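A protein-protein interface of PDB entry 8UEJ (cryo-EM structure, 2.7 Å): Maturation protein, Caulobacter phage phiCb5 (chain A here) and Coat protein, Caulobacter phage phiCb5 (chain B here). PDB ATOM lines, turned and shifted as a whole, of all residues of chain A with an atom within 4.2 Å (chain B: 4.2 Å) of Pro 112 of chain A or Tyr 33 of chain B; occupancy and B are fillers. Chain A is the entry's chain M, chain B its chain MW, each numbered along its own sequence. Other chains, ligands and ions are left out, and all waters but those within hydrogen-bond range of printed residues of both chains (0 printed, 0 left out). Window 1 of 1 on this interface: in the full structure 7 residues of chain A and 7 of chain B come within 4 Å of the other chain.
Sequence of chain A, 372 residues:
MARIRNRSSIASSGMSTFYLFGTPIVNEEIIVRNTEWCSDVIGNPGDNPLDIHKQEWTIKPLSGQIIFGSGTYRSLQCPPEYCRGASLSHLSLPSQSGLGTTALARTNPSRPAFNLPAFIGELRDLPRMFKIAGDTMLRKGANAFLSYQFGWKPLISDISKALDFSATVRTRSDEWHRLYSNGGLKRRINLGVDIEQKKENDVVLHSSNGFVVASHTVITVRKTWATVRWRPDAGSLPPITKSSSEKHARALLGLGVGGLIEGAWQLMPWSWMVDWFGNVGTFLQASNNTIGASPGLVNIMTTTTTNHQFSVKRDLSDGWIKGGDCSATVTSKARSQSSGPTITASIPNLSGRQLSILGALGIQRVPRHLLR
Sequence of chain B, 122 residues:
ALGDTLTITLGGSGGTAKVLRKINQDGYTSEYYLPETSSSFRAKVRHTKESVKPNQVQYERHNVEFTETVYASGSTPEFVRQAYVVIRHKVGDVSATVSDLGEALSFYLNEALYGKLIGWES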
ATOM      1  N   SER A 110      14.971   8.123 -15.352  1.00  0.00           N
ATOM      2  CA  SER A 110      15.476   9.391 -15.858  1.00  0.00           C
ATOM      3  C   SER A 110      15.179  10.496 -14.852  1.00  0.00           C
ATOM      4  O   SER A 110      14.100  10.539 -14.253  1.00  0.00           O
ATOM      5  CB  SER A 110      14.849   9.746 -17.207  1.00  0.00           C
ATOM      6  OG  SER A 110      13.444   9.911 -17.110  1.00  0.00           O
ATOM      7  N   ARG A 111      16.140  11.392 -14.664  1.00  0.00           N
ATOM      8  CA  ARG A 111      15.995  12.490 -13.720  1.00  0.00           C
ATOM      9  C   ARG A 111      17.002  13.573 -14.084  1.00  0.00           C
ATOM     10  O   ARG A 111      18.007  13.291 -14.745  1.00  0.00           O
ATOM     11  CB  ARG A 111      16.203  12.001 -12.279  1.00  0.00           C
ATOM     12  CG  ARG A 111      17.566  11.383 -12.075  1.00  0.00           C
ATOM     13  CD  ARG A 111      17.745  10.803 -10.684  1.00  0.00           C
ATOM     14  NE  ARG A 111      16.799   9.738 -10.364  1.00  0.00           N
ATOM     15  CZ  ARG A 111      15.730   9.890  -9.592  1.00  0.00           C
ATOM     16  NH1 ARG A 111      15.380  11.078  -9.114  1.00  0.00           N
ATOM     17  NH2 ARG A 111      14.990   8.826  -9.293  1.00  0.00           N
ATOM     18  N   PRO A 112      16.766  14.819 -13.668  1.00  0.00           N
ATOM     19  CA  PRO A 112      17.648  15.913 -14.092  1.00  0.00           C
ATOM     20  C   PRO A 112      19.068  15.736 -13.570  1.00  0.00           C
ATOM     21  O   PRO A 112      19.306  15.032 -12.589  1.00  0.00           O
ATOM     22  CB  PRO A 112      16.971  17.159 -13.505  1.00  0.00           C
ATOM     23  CG  PRO A 112      16.140  16.653 -12.396  1.00  0.00           C
ATOM     24  CD  PRO A 112      15.642  15.323 -12.862  1.00  0.00           C
ATOM     25  N   ALA A 113      20.021  16.370 -14.259  1.00  0.00           N
ATOM     26  CA  ALA A 113      21.443  16.217 -13.975  1.00  0.00           C
ATOM     27  C   ALA A 113      22.061  17.566 -13.639  1.00  0.00           C
ATOM     28  O   ALA A 113      21.491  18.627 -13.909  1.00  0.00           O
ATOM     29  CB  ALA A 113      22.193  15.596 -15.163  1.00  0.00           C
ATOM     30  N   LEU B  20       4.221  15.337 -17.942  1.00  0.00           N
ATOM     31  CA  LEU B  20       5.275  14.993 -16.997  1.00  0.00           C
ATOM     32  C   LEU B  20       4.944  13.692 -16.268  1.00  0.00           C
ATOM     33  O   LEU B  20       3.792  13.254 -16.219  1.00  0.00           O
ATOM     34  CB  LEU B  20       5.481  16.123 -15.985  1.00  0.00           C
ATOM     35  CG  LEU B  20       5.488  17.567 -16.492  1.00  0.00           C
ATOM     36  CD1 LEU B  20       5.971  18.485 -15.385  1.00  0.00           C
ATOM     37  CD2 LEU B  20       6.381  17.720 -17.712  1.00  0.00           C
ATOM     38  N   ARG B  21       5.978  13.070 -15.699  1.00  0.00           N
ATOM     39  CA  ARG B  21       5.848  11.771 -15.049  1.00  0.00           C
ATOM     40  C   ARG B  21       6.052  11.906 -13.545  1.00  0.00           C
ATOM     41  O   ARG B  21       6.908  12.673 -13.094  1.00  0.00           O
ATOM     42  CB  ARG B  21       6.857  10.764 -15.605  1.00  0.00           C
ATOM     43  CG  ARG B  21       6.549  10.290 -17.020  1.00  0.00           C
ATOM     44  CD  ARG B  21       7.809  10.293 -17.881  1.00  0.00           C
ATOM     45  NE  ARG B  21       8.947   9.748 -17.150  1.00  0.00           N
ATOM     46  CZ  ARG B  21      10.187   9.685 -17.617  1.00  0.00           C
ATOM     47  NH1 ARG B  21      10.513  10.197 -18.794  1.00  0.00           N
ATOM     48  NH2 ARG B  21      11.127   9.096 -16.879  1.00  0.00           N
ATOM     49  N   GLU B  31       6.311  15.450  -6.955  1.00  0.00           N
ATOM     50  CA  GLU B  31       7.024  16.170  -7.997  1.00  0.00           C
ATOM     51  C   GLU B  31       6.945  15.380  -9.294  1.00  0.00           C
ATOM     52  O   GLU B  31       6.893  14.148  -9.279  1.00  0.00           O
ATOM     53  CB  GLU B  31       8.484  16.411  -7.593  1.00  0.00           C
ATOM     54  CG  GLU B  31       9.267  17.265  -8.573  1.00  0.00           C
ATOM     55  CD  GLU B  31      10.094  16.450  -9.537  1.00  0.00           C
ATOM     56  OE1 GLU B  31      10.617  15.395  -9.125  1.00  0.00           O
ATOM     57  OE2 GLU B  31      10.227  16.863 -10.707  1.00  0.00           O
ATOM     58  N   TYR B  32       6.923  16.102 -10.410  1.00  0.00           N
ATOM     59  CA  TYR B  32       6.827  15.516 -11.738  1.00  0.00           C
ATOM     60  C   TYR B  32       7.979  16.027 -12.594  1.00  0.00           C
ATOM     61  O   TYR B  32       8.394  17.184 -12.472  1.00  0.00           O
ATOM     62  CB  TYR B  32       5.503  15.875 -12.419  1.00  0.00           C
ATOM     63  CG  TYR B  32       4.272  15.272 -11.795  1.00  0.00           C
ATOM     64  CD1 TYR B  32       3.806  15.713 -10.567  1.00  0.00           C
ATOM     65  CD2 TYR B  32       3.554  14.287 -12.447  1.00  0.00           C
ATOM     66  CE1 TYR B  32       2.672  15.173 -10.002  1.00  0.00           C
ATOM     67  CE2 TYR B  32       2.420  13.745 -11.890  1.00  0.00           C
ATOM     68  CZ  TYR B  32       1.983  14.191 -10.669  1.00  0.00           C
ATOM     69  OH  TYR B  32       0.849  13.650 -10.103  1.00  0.00           O
ATOM     70  N   TYR B  33       8.480  15.164 -13.477  1.00  0.00           N
ATOM     71  CA  TYR B  33       9.609  15.523 -14.324  1.00  0.00           C
ATOM     72  C   TYR B  33       9.478  14.838 -15.677  1.00  0.00           C
ATOM     73  O   TYR B  33       8.779  13.832 -15.826  1.00  0.00           O
ATOM     74  CB  TYR B  33      10.942  15.153 -13.661  1.00  0.00           C
ATOM     75  CG  TYR B  33      12.142  15.325 -14.562  1.00  0.00           C
ATOM     76  CD1 TYR B  33      12.636  16.584 -14.848  1.00  0.00           C
ATOM     77  CD2 TYR B  33      12.774  14.227 -15.132  1.00  0.00           C
ATOM     78  CE1 TYR B  33      13.724  16.750 -15.670  1.00  0.00           C
ATOM     79  CE2 TYR B  33      13.867  14.387 -15.957  1.00  0.00           C
ATOM     80  CZ  TYR B  33      14.338  15.652 -16.222  1.00  0.00           C
ATOM     81  OH  TYR B  33      15.427  15.825 -17.048  1.00  0.00           O
ATOM     82  N   LEU B  34      10.154  15.414 -16.672  1.00  0.00           N
ATOM     83  CA  LEU B  34      10.213  14.864 -18.021  1.00  0.00           C
ATOM     84  C   LEU B  34      11.473  15.365 -18.721  1.00  0.00           C
ATOM     85  O   LEU B  34      11.703  16.580 -18.772  1.00  0.00           O
ATOM     86  CB  LEU B  34       8.977  15.265 -18.826  1.00  0.00           C
ATOM     87  CG  LEU B  34       8.985  14.822 -20.289  1.00  0.00           C
ATOM     88  CD1 LEU B  34       7.624  14.272 -20.678  1.00  0.00           C
ATOM     89  CD2 LEU B  34       9.384  15.976 -21.203  1.00  0.00           C
ATOM     90  N   PRO B  35      12.315  14.487 -19.258  1.00  0.00           N
ATOM     91  CA  PRO B  35      13.507  14.954 -19.968  1.00  0.00           C
ATOM     92  C   PRO B  35      13.234  15.210 -21.445  1.00  0.00           C
ATOM     93  O   PRO B  35      12.423  14.539 -22.084  1.00  0.00           O
ATOM     94  CB  PRO B  35      14.492  13.800 -19.776  1.00  0.00           C
ATOM     95  CG  PRO B  35      13.623  12.597 -19.753  1.00  0.00           C
ATOM     96  CD  PRO B  35      12.305  13.019 -19.132  1.00  0.00           C
ATOM     97  N   SER B  40      14.066  20.626 -20.260  1.00  0.00           N
ATOM     98  CA  SER B  40      13.414  19.710 -19.333  1.00  0.00           C
ATOM     99  C   SER B  40      12.277  20.448 -18.635  1.00  0.00           C
ATOM    100  O   SER B  40      12.287  21.677 -18.530  1.00  0.00           O
ATOM    101  CB  SER B  40      14.410  19.164 -18.307  1.00  0.00           C
ATOM    102  OG  SER B  40      14.965  20.217 -17.530  1.00  0.00           O
ATOM    103  N   PHE B  41      11.310  19.682 -18.134  1.00  0.00           N
ATOM    104  CA  PHE B  41      10.132  20.231 -17.468  1.00  0.00           C
ATOM    105  C   PHE B  41      10.039  19.699 -16.044  1.00  0.00           C
ATOM    106  O   PHE B  41      10.160  18.490 -15.819  1.00  0.00           O
ATOM    107  CB  PHE B  41       8.853  19.900 -18.246  1.00  0.00           C
ATOM    108  CG  PHE B  41       8.815  20.492 -19.626  1.00  0.00           C
ATOM    109  CD1 PHE B  41       9.487  19.900 -20.675  1.00  0.00           C
ATOM    110  CD2 PHE B  41       8.120  21.662 -19.861  1.00  0.00           C
ATOM    111  CE1 PHE B  41       9.453  20.461 -21.936  1.00  0.00           C
ATOM    112  CE2 PHE B  41       8.087  22.220 -21.116  1.00  0.00           C
ATOM    113  CZ  PHE B  41       8.753  21.619 -22.152  1.00  0.00           C
ATOM    114  N   ARG B  42       9.805  20.606 -15.094  1.00  0.00           N
ATOM    115  CA  ARG B  42       9.768  20.297 -13.669  1.00  0.00           C
ATOM    116  C   ARG B  42       8.507  20.880 -13.047  1.00  0.00           C
ATOM    117  O   ARG B  42       8.234  22.073 -13.204  1.00  0.00           O
ATOM    118  CB  ARG B  42      11.001  20.861 -12.951  1.00  0.00           C
ATOM    119  CG  ARG B  42      11.076  20.483 -11.479  1.00  0.00           C
ATOM    120  CD  ARG B  42      12.318  21.014 -10.753  1.00  0.00           C
ATOM    121  NE  ARG B  42      13.584  20.473 -11.244  1.00  0.00           N
ATOM    122  CZ  ARG B  42      14.523  21.174 -11.872  1.00  0.00           C
ATOM    123  NH1 ARG B  42      14.392  22.472 -12.098  1.00  0.00           N
ATOM    124  NH2 ARG B  42      15.636  20.560 -12.270  1.00  0.00           N
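The guanidinium group of Arg 21 of chain B lies within hydrogen-bond range of the side-chain hydroxyl of Ser 110 of chain A.
Of the printed residues of chain B, Arg 111 of chain A touches Tyr 33 (3.6 Å).
Pro 112 of chain A touches just these residues of chain B: Tyr 33 (3.6 Å) and Arg 42 (3.9 Å).
Printed residues of chain A within 4 Å of Arg 21 of chain B: Ser 110.
Of the printed residues of chain A, Tyr 33 of chain B touches Arg 111 and Pro 112.
Of the printed residues of chain A, Pro 35 of chain B touches Ser 110 (3.8 Å).
The nearest printed residue of chain A that does not touch Tyr 33 of chain B is Ser 110 of chain A (4.02 Å).
The backbone NH of Arg 21 of chain B is in hydrogen-bond range of the backbone carbonyl oxygen of Tyr 33 of chain B, at 2.9 Å.
CG of Pro 35 of chain B touches OG of Ser 110 of chain A (3.8 Å).
Arg 111 of chain A touches Tyr 33 of chain B.
CD of Pro 112 of chain A touches CZ of Tyr 33 of chain B, at 3.6 Å.
NH2 of Arg 42 of chain B touches CB of Pro 112 of chain A, 3.9 Å away.
Hydrophobic or aromatic side chains of chain B that line the printed part of chain A: Tyr 33 and Pro 35.
Of the 4 printed residues of chain A, 3 touch a printed residue of chain B.
Among the printed residues, 5 pairs touch across the chains.
Among the printed residues, no Asp or Glu carboxylate lies within 4 Å of a Lys or Arg side-chain nitrogen of the other chain.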
